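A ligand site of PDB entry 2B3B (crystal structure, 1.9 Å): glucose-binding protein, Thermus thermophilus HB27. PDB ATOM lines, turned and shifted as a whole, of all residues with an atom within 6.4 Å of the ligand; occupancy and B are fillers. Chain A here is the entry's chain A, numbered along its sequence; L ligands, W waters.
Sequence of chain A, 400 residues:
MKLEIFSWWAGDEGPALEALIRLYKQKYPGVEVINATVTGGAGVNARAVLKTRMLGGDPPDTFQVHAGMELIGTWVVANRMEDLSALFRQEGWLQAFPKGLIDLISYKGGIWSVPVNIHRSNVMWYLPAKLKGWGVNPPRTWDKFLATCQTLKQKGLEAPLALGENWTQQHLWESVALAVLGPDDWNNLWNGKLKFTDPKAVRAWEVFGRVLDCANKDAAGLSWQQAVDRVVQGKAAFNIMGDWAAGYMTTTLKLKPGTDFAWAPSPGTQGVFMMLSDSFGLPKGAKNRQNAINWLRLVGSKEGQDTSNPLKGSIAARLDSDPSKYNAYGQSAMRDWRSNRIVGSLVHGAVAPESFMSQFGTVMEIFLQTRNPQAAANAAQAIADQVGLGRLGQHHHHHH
Water W1 lies within hydrogen-bond range of the side-chain amino group (NZ) of Lys 312, the side-chain carboxylate (OE2) of Glu 13 and an oxygen (O4) of the ligand.
A ring nitrogen (ND1) of His 66 lies close to the backbone carbonyl oxygen (O) of His 348 (3.3 Å).
The side-chain amide nitrogen of Gln 64 is in hydrogen-bond range of the side-chain carboxylate of Asp 278, at 3.1 Å.
The side-chain amide oxygen (OD1) of Asn 117 is in hydrogen-bond range of the backbone NH (N) of Asp 278, 2.8 Å away.
The side-chain carboxylate (OE1) of Glu 13 sits at hydrogen-bond distance from the indole nitrogen (NE1) of Trp 224 (3.1 Å).
A ring nitrogen (NE2) of His 119 lies within hydrogen-bond range of the side-chain amino group (NZ) of Lys 312 (2.9 Å).
The indole nitrogen (NE1) of Trp 9 lies close to the side-chain amide nitrogen (NE2) of Gln 64.
The backbone carbonyl oxygen of Leu 276 is in hydrogen-bond range of the backbone NH of His 119 (2.9 Å).
The indole nitrogen (NE1) of Trp 244 is in hydrogen-bond range of the side-chain sulfur (SD) of Met 241 (3.3 Å).
Residues that only touch the ligand: Leu 276 (3.2 Å), Trp 244 (3.5 Å), Gln 64 (3.6 Å), Gly 41 (3.7 Å) and Trp 224 (3.7 Å).
Hydrophobic or aromatic side chains within 4 Å of the ligand: Trp 8, Trp 9, Ala 42, His 66, Trp 244, Leu 276 and His 348.
13 residues have an atom within 4 Å of the ligand: Trp 8, Trp 9, Glu 13, Gly 41, Ala 42, Gln 64, His 66, Trp 224, Trp 244, Leu 276, Asp 278, Lys 312 and His 348.
The nearest printed residue that does not touch the ligand is His 119 (4.002 Å).
O1 of the ligand sits at hydrogen-bond distance from ND1 of His 348, at 2.4 Å.
The side-chain carboxylate (OD1) of Asp 278 lies within hydrogen-bond range of an oxygen (O2) of the ligand, 2.6 Å away.
O4 of the ligand is in hydrogen-bond range of OE2 of Glu 13 (2.6 Å).
An oxygen (O2) of the ligand lies within hydrogen-bond range of a ring nitrogen (NE2) of His 66.
An oxygen (O4) of the ligand is in hydrogen-bond range of the side-chain amino group (NZ) of Lys 312 (2.8 Å).
O3 of the ligand lies within hydrogen-bond range of NE1 of Trp 9 (2.9 Å).
An oxygen (O6) of the ligand is in hydrogen-bond range of the backbone NH of Ala 42 (3.0 Å).
The indole nitrogen (NE1) of Trp 8 sits close to an oxygen (O6) of the ligand, at 3.4 Å.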
ATOM      1  N   TRP A   8       3.723  28.011  22.642  1.00  0.00           N
ATOM      2  CA  TRP A   8       4.326  28.868  23.641  1.00  0.00           C
ATOM      3  C   TRP A   8       5.706  28.386  24.047  1.00  0.00           C
ATOM      4  O   TRP A   8       6.212  28.696  25.120  1.00  0.00           O
ATOM      5  CB  TRP A   8       3.386  29.072  24.827  1.00  0.00           C
ATOM      6  CG  TRP A   8       2.932  27.922  25.641  1.00  0.00           C
ATOM      7  CD1 TRP A   8       3.492  27.460  26.785  1.00  0.00           C
ATOM      8  CD2 TRP A   8       1.718  27.190  25.469  1.00  0.00           C
ATOM      9  NE1 TRP A   8       2.733  26.447  27.336  1.00  0.00           N
ATOM     10  CE2 TRP A   8       1.621  26.273  26.555  1.00  0.00           C
ATOM     11  CE3 TRP A   8       0.684  27.225  24.523  1.00  0.00           C
ATOM     12  CZ2 TRP A   8       0.542  25.381  26.692  1.00  0.00           C
ATOM     13  CZ3 TRP A   8      -0.396  26.323  24.661  1.00  0.00           C
ATOM     14  CH2 TRP A   8      -0.443  25.415  25.729  1.00  0.00           C
ATOM     15  N   TRP A   9       6.349  27.650  23.146  1.00  0.00           N
ATOM     16  CA  TRP A   9       7.641  27.075  23.489  1.00  0.00           C
ATOM     17  C   TRP A   9       8.770  28.048  23.182  1.00  0.00           C
ATOM     18  O   TRP A   9       9.641  27.780  22.348  1.00  0.00           O
ATOM     19  CB  TRP A   9       7.815  25.737  22.789  1.00  0.00           C
ATOM     20  CG  TRP A   9       6.954  24.698  23.377  1.00  0.00           C
ATOM     21  CD1 TRP A   9       6.598  24.562  24.709  1.00  0.00           C
ATOM     22  CD2 TRP A   9       6.331  23.618  22.681  1.00  0.00           C
ATOM     23  NE1 TRP A   9       5.766  23.479  24.855  1.00  0.00           N
ATOM     24  CE2 TRP A   9       5.605  22.858  23.642  1.00  0.00           C
ATOM     25  CE3 TRP A   9       6.290  23.213  21.337  1.00  0.00           C
ATOM     26  CZ2 TRP A   9       4.871  21.734  23.305  1.00  0.00           C
ATOM     27  CZ3 TRP A   9       5.559  22.087  20.991  1.00  0.00           C
ATOM     28  CH2 TRP A   9       4.852  21.357  21.973  1.00  0.00           C
ATOM     29  N   GLU A  13      12.239  27.053  26.672  1.00  0.00           N
ATOM     30  CA  GLU A  13      11.309  25.981  26.368  1.00  0.00           C
ATOM     31  C   GLU A  13      11.417  25.501  24.905  1.00  0.00           C
ATOM     32  O   GLU A  13      10.778  24.519  24.538  1.00  0.00           O
ATOM     33  CB  GLU A  13       9.871  26.411  26.658  1.00  0.00           C
ATOM     34  CG  GLU A  13       9.627  26.835  28.121  1.00  0.00           C
ATOM     35  CD  GLU A  13       8.250  26.439  28.622  1.00  0.00           C
ATOM     36  OE1 GLU A  13       7.502  27.310  29.143  1.00  0.00           O
ATOM     37  OE2 GLU A  13       7.925  25.243  28.493  1.00  0.00           O
ATOM     38  N   GLY A  40       5.045  33.002  27.171  1.00  0.00           N
ATOM     39  CA  GLY A  40       4.221  32.972  28.386  1.00  0.00           C
ATOM     40  C   GLY A  40       3.969  31.577  28.885  1.00  0.00           C
ATOM     41  O   GLY A  40       3.397  30.732  28.172  1.00  0.00           O
ATOM     42  N   GLY A  41       4.351  31.339  30.142  1.00  0.00           N
ATOM     43  CA  GLY A  41       4.145  30.076  30.779  1.00  0.00           C
ATOM     44  C   GLY A  41       2.730  29.548  30.685  1.00  0.00           C
ATOM     45  O   GLY A  41       1.764  30.306  30.806  1.00  0.00           O
ATOM     46  N   ALA A  42       2.628  28.243  30.456  1.00  0.00           N
ATOM     47  CA  ALA A  42       1.380  27.514  30.412  1.00  0.00           C
ATOM     48  C   ALA A  42       0.363  27.999  29.395  1.00  0.00           C
ATOM     49  O   ALA A  42      -0.817  27.668  29.509  1.00  0.00           O
ATOM     50  CB  ALA A  42       0.744  27.434  31.836  1.00  0.00           C
ATOM     51  N   GLY A  43       0.800  28.781  28.412  1.00  0.00           N
ATOM     52  CA  GLY A  43      -0.077  29.168  27.320  1.00  0.00           C
ATOM     53  C   GLY A  43      -1.150  30.223  27.595  1.00  0.00           C
ATOM     54  O   GLY A  43      -2.041  30.422  26.769  1.00  0.00           O
ATOM     55  N   ARG A  47      -3.017  31.425  24.288  1.00  0.00           N
ATOM     56  CA  ARG A  47      -4.493  31.319  24.275  1.00  0.00           C
ATOM     57  C   ARG A  47      -5.145  32.635  23.790  1.00  0.00           C
ATOM     58  O   ARG A  47      -6.024  32.639  22.910  1.00  0.00           O
ATOM     59  CB  ARG A  47      -4.909  30.963  25.716  1.00  0.00           C
ATOM     60  CG  ARG A  47      -6.310  30.464  26.026  1.00  0.00           C
ATOM     61  CD  ARG A  47      -6.255  29.690  27.410  1.00  0.00           C
ATOM     62  NE  ARG A  47      -5.427  28.475  27.280  1.00  0.00           N
ATOM     63  CZ  ARG A  47      -4.560  28.004  28.182  1.00  0.00           C
ATOM     64  NH1 ARG A  47      -4.294  28.646  29.317  1.00  0.00           N
ATOM     65  NH2 ARG A  47      -3.863  26.906  27.892  1.00  0.00           N
ATOM     66  N   GLN A  64      -0.177  24.483  19.109  1.00  0.00           N
ATOM     67  CA  GLN A  64      -0.066  23.741  20.345  1.00  0.00           C
ATOM     68  C   GLN A  64      -1.385  23.851  21.108  1.00  0.00           C
ATOM     69  O   GLN A  64      -1.940  24.923  21.257  1.00  0.00           O
ATOM     70  CB  GLN A  64       1.052  24.334  21.196  1.00  0.00           C
ATOM     71  CG  GLN A  64       1.344  23.581  22.460  1.00  0.00           C
ATOM     72  CD  GLN A  64       2.373  24.270  23.361  1.00  0.00           C
ATOM     73  OE1 GLN A  64       3.048  25.205  22.958  1.00  0.00           O
ATOM     74  NE2 GLN A  64       2.486  23.803  24.587  1.00  0.00           N
ATOM     75  N   HIS A  66      -3.766  21.601  24.315  1.00  0.00           N
ATOM     76  CA  HIS A  66      -3.857  20.541  25.260  1.00  0.00           C
ATOM     77  C   HIS A  66      -4.947  19.551  24.867  1.00  0.00           C
ATOM     78  O   HIS A  66      -6.085  19.958  24.563  1.00  0.00           O
ATOM     79  CB  HIS A  66      -4.113  21.065  26.678  1.00  0.00           C
ATOM     80  CG  HIS A  66      -2.933  21.749  27.296  1.00  0.00           C
ATOM     81  ND1 HIS A  66      -2.975  23.008  27.829  1.00  0.00           N
ATOM     82  CD2 HIS A  66      -1.655  21.324  27.435  1.00  0.00           C
ATOM     83  CE1 HIS A  66      -1.784  23.341  28.296  1.00  0.00           C
ATOM     84  NE2 HIS A  66      -0.975  22.325  28.089  1.00  0.00           N
ATOM     85  N   ASN A 117       3.373  14.258  23.289  1.00  0.00           N
ATOM     86  CA  ASN A 117       4.002  13.984  24.558  1.00  0.00           C
ATOM     87  C   ASN A 117       2.985  13.707  25.641  1.00  0.00           C
ATOM     88  O   ASN A 117       1.772  13.800  25.417  1.00  0.00           O
ATOM     89  CB  ASN A 117       4.904  15.166  24.959  1.00  0.00           C
ATOM     90  CG  ASN A 117       4.139  16.429  25.388  1.00  0.00           C
ATOM     91  OD1 ASN A 117       2.916  16.409  25.545  1.00  0.00           O
ATOM     92  ND2 ASN A 117       4.860  17.528  25.598  1.00  0.00           N
ATOM     93  N   HIS A 119       3.100  15.124  29.717  1.00  0.00           N
ATOM     94  CA  HIS A 119       3.713  15.745  30.893  1.00  0.00           C
ATOM     95  C   HIS A 119       2.949  15.327  32.139  1.00  0.00           C
ATOM     96  O   HIS A 119       1.766  15.016  32.087  1.00  0.00           O
ATOM     97  CB  HIS A 119       3.717  17.287  30.831  1.00  0.00           C
ATOM     98  CG  HIS A 119       4.889  17.890  30.118  1.00  0.00           C
ATOM     99  ND1 HIS A 119       6.179  17.782  30.573  1.00  0.00           N
ATOM    100  CD2 HIS A 119       4.942  18.658  29.004  1.00  0.00           C
ATOM    101  CE1 HIS A 119       6.988  18.431  29.756  1.00  0.00           C
ATOM    102  NE2 HIS A 119       6.261  18.969  28.789  1.00  0.00           N
ATOM    103  N   TRP A 167      -0.510  31.366  37.475  1.00  0.00           N
ATOM    104  CA  TRP A 167      -0.805  30.001  36.972  1.00  0.00           C
ATOM    105  C   TRP A 167      -0.029  28.948  37.765  1.00  0.00           C
ATOM    106  O   TRP A 167      -0.512  27.826  37.967  1.00  0.00           O
ATOM    107  CB  TRP A 167      -0.589  29.881  35.441  1.00  0.00           C
ATOM    108  CG  TRP A 167       0.798  29.756  34.970  1.00  0.00           C
ATOM    109  CD1 TRP A 167       1.604  30.749  34.491  1.00  0.00           C
ATOM    110  CD2 TRP A 167       1.590  28.567  34.983  1.00  0.00           C
ATOM    111  NE1 TRP A 167       2.843  30.242  34.185  1.00  0.00           N
ATOM    112  CE2 TRP A 167       2.860  28.909  34.459  1.00  0.00           C
ATOM    113  CE3 TRP A 167       1.339  27.240  35.384  1.00  0.00           C
ATOM    114  CZ2 TRP A 167       3.885  27.961  34.308  1.00  0.00           C
ATOM    115  CZ3 TRP A 167       2.349  26.303  35.216  1.00  0.00           C
ATOM    116  CH2 TRP A 167       3.614  26.666  34.685  1.00  0.00           C
ATOM    117  N   TRP A 224       7.974  30.381  35.938  1.00  0.00           N
ATOM    118  CA  TRP A 224       8.121  29.058  36.486  1.00  0.00           C
ATOM    119  C   TRP A 224       9.591  28.697  36.535  1.00  0.00           C
ATOM    120  O   TRP A 224      10.000  28.076  37.491  1.00  0.00           O
ATOM    121  CB  TRP A 224       7.279  27.978  35.775  1.00  0.00           C
ATOM    122  CG  TRP A 224       7.731  27.608  34.411  1.00  0.00           C
ATOM    123  CD1 TRP A 224       7.258  28.080  33.239  1.00  0.00           C
ATOM    124  CD2 TRP A 224       8.756  26.667  34.077  1.00  0.00           C
ATOM    125  NE1 TRP A 224       7.913  27.496  32.185  1.00  0.00           N
ATOM    126  CE2 TRP A 224       8.845  26.630  32.672  1.00  0.00           C
ATOM    127  CE3 TRP A 224       9.612  25.861  34.838  1.00  0.00           C
ATOM    128  CZ2 TRP A 224       9.761  25.819  32.000  1.00  0.00           C
ATOM    129  CZ3 TRP A 224      10.528  25.051  34.166  1.00  0.00           C
ATOM    130  CH2 TRP A 224      10.604  25.046  32.750  1.00  0.00           C
ATOM    131  N   MET A 241       5.872  21.524  40.319  1.00  0.00           N
ATOM    132  CA  MET A 241       5.811  21.949  38.926  1.00  0.00           C
ATOM    133  C   MET A 241       5.830  20.761  37.966  1.00  0.00           C
ATOM    134  O   MET A 241       6.353  19.688  38.309  1.00  0.00           O
ATOM    135  CB  MET A 241       7.000  22.872  38.637  1.00  0.00           C
ATOM    136  CG  MET A 241       6.986  23.613  37.304  1.00  0.00           C
ATOM    137  SD  MET A 241       5.384  24.309  36.796  1.00  0.00           S
ATOM    138  CE  MET A 241       4.967  25.337  38.215  1.00  0.00           C
ATOM    139  N   TRP A 244       8.339  19.606  32.640  1.00  0.00           N
ATOM    140  CA  TRP A 244       9.134  20.541  31.860  1.00  0.00           C
ATOM    141  C   TRP A 244      10.307  21.122  32.699  1.00  0.00           C
ATOM    142  O   TRP A 244      11.325  21.571  32.148  1.00  0.00           O
ATOM    143  CB  TRP A 244       8.274  21.657  31.273  1.00  0.00           C
ATOM    144  CG  TRP A 244       7.303  22.298  32.215  1.00  0.00           C
ATOM    145  CD1 TRP A 244       7.521  23.387  33.003  1.00  0.00           C
ATOM    146  CD2 TRP A 244       5.949  21.902  32.435  1.00  0.00           C
ATOM    147  NE1 TRP A 244       6.387  23.701  33.722  1.00  0.00           N
ATOM    148  CE2 TRP A 244       5.405  22.790  33.392  1.00  0.00           C
ATOM    149  CE3 TRP A 244       5.133  20.872  31.914  1.00  0.00           C
ATOM    150  CZ2 TRP A 244       4.080  22.695  33.840  1.00  0.00           C
ATOM    151  CZ3 TRP A 244       3.832  20.771  32.351  1.00  0.00           C
ATOM    152  CH2 TRP A 244       3.311  21.676  33.311  1.00  0.00           C
ATOM    153  N   LEU A 276      -1.085  15.622  31.474  1.00  0.00           N
ATOM    154  CA  LEU A 276      -1.524  16.513  30.414  1.00  0.00           C
ATOM    155  C   LEU A 276      -0.776  16.130  29.148  1.00  0.00           C
ATOM    156  O   LEU A 276       0.213  15.432  29.204  1.00  0.00           O
ATOM    157  CB  LEU A 276      -1.255  17.985  30.760  1.00  0.00           C
ATOM    158  CG  LEU A 276       0.216  18.276  31.079  1.00  0.00           C
ATOM    159  CD1 LEU A 276       0.747  19.347  30.166  1.00  0.00           C
ATOM    160  CD2 LEU A 276       0.502  18.591  32.572  1.00  0.00           C
ATOM    161  N   SER A 277      -1.214  16.641  28.012  1.00  0.00           N
ATOM    162  CA  SER A 277      -0.606  16.294  26.736  1.00  0.00           C
ATOM    163  C   SER A 277      -0.644  17.491  25.788  1.00  0.00           C
ATOM    164  O   SER A 277      -1.709  18.093  25.512  1.00  0.00           O
ATOM    165  CB  SER A 277      -1.324  15.080  26.133  1.00  0.00           C
ATOM    166  OG  SER A 277      -0.713  14.661  24.936  1.00  0.00           O
ATOM    167  N   ASP A 278       0.545  17.842  25.289  1.00  0.00           N
ATOM    168  CA  ASP A 278       0.660  18.785  24.193  1.00  0.00           C
ATOM    169  C   ASP A 278       0.365  18.083  22.868  1.00  0.00           C
ATOM    170  O   ASP A 278       0.895  17.001  22.607  1.00  0.00           O
ATOM    171  CB  ASP A 278       2.061  19.372  24.165  1.00  0.00           C
ATOM    172  CG  ASP A 278       2.382  20.203  25.410  1.00  0.00           C
ATOM    173  OD1 ASP A 278       1.570  21.094  25.757  1.00  0.00           O
ATOM    174  OD2 ASP A 278       3.451  19.961  26.012  1.00  0.00           O
ATOM    175  N   LYS A 312      12.792  17.908  26.290  1.00  0.00           N
ATOM    176  CA  LYS A 312      11.651  18.584  26.936  1.00  0.00           C
ATOM    177  C   LYS A 312      11.415  18.250  28.420  1.00  0.00           C
ATOM    178  O   LYS A 312      10.931  19.098  29.158  1.00  0.00           O
ATOM    179  CB  LYS A 312      10.405  18.265  26.109  1.00  0.00           C
ATOM    180  CG  LYS A 312       9.122  19.005  26.484  1.00  0.00           C
ATOM    181  CD  LYS A 312       9.142  20.397  26.008  1.00  0.00           C
ATOM    182  CE  LYS A 312       7.730  20.975  25.978  1.00  0.00           C
ATOM    183  NZ  LYS A 312       7.290  21.274  27.370  1.00  0.00           N
ATOM    184  N   VAL A 347      -5.082  22.792  35.194  1.00  0.00           N
ATOM    185  CA  VAL A 347      -4.360  23.971  34.759  1.00  0.00           C
ATOM    186  C   VAL A 347      -3.828  23.794  33.340  1.00  0.00           C
ATOM    187  O   VAL A 347      -3.690  24.779  32.596  1.00  0.00           O
ATOM    188  CB  VAL A 347      -3.247  24.368  35.753  1.00  0.00           C
ATOM    189  CG1 VAL A 347      -2.432  25.539  35.232  1.00  0.00           C
ATOM    190  CG2 VAL A 347      -3.902  24.753  37.092  1.00  0.00           C
ATOM    191  N   HIS A 348      -3.627  22.535  32.965  1.00  0.00           N
ATOM    192  CA  HIS A 348      -3.079  22.194  31.647  1.00  0.00           C
ATOM    193  C   HIS A 348      -4.076  21.438  30.749  1.00  0.00           C
ATOM    194  O   HIS A 348      -3.661  20.593  29.935  1.00  0.00           O
ATOM    195  CB  HIS A 348      -1.747  21.497  31.824  1.00  0.00           C
ATOM    196  CG  HIS A 348      -0.804  22.260  32.694  1.00  0.00           C
ATOM    197  ND1 HIS A 348      -0.101  23.370  32.255  1.00  0.00           N
ATOM    198  CD2 HIS A 348      -0.534  22.145  34.019  1.00  0.00           C
ATOM    199  CE1 HIS A 348       0.604  23.859  33.262  1.00  0.00           C
ATOM    200  NE2 HIS A 348       0.334  23.150  34.348  1.00  0.00           N
HETATM  201  C1  LIG L   1       2.068  23.965  29.354  1.00  0.00           C
HETATM  202  C2  LIG L   1       2.544  22.857  28.343  1.00  0.00           C
HETATM  203  C3  LIG L   1       4.045  22.511  28.399  1.00  0.00           C
HETATM  204  C4  LIG L   1       4.877  23.704  28.851  1.00  0.00           C
HETATM  205  C5  LIG L   1       4.376  24.236  30.210  1.00  0.00           C
HETATM  206  C6  LIG L   1       5.113  25.477  30.740  1.00  0.00           C
HETATM  207  O1  LIG L   1       0.925  23.666  30.081  1.00  0.00           O
HETATM  208  O2  LIG L   1       1.676  21.717  28.232  1.00  0.00           O
HETATM  209  O3  LIG L   1       4.447  22.149  27.092  1.00  0.00           O
HETATM  210  O4  LIG L   1       6.244  23.332  28.976  1.00  0.00           O
HETATM  211  O5  LIG L   1       3.000  24.604  30.201  1.00  0.00           O
HETATM  212  O6  LIG L   1       5.003  26.553  29.856  1.00  0.00           O
HETATM  213  O   HOH W   1       9.359  22.993  27.870  1.00  0.00           O
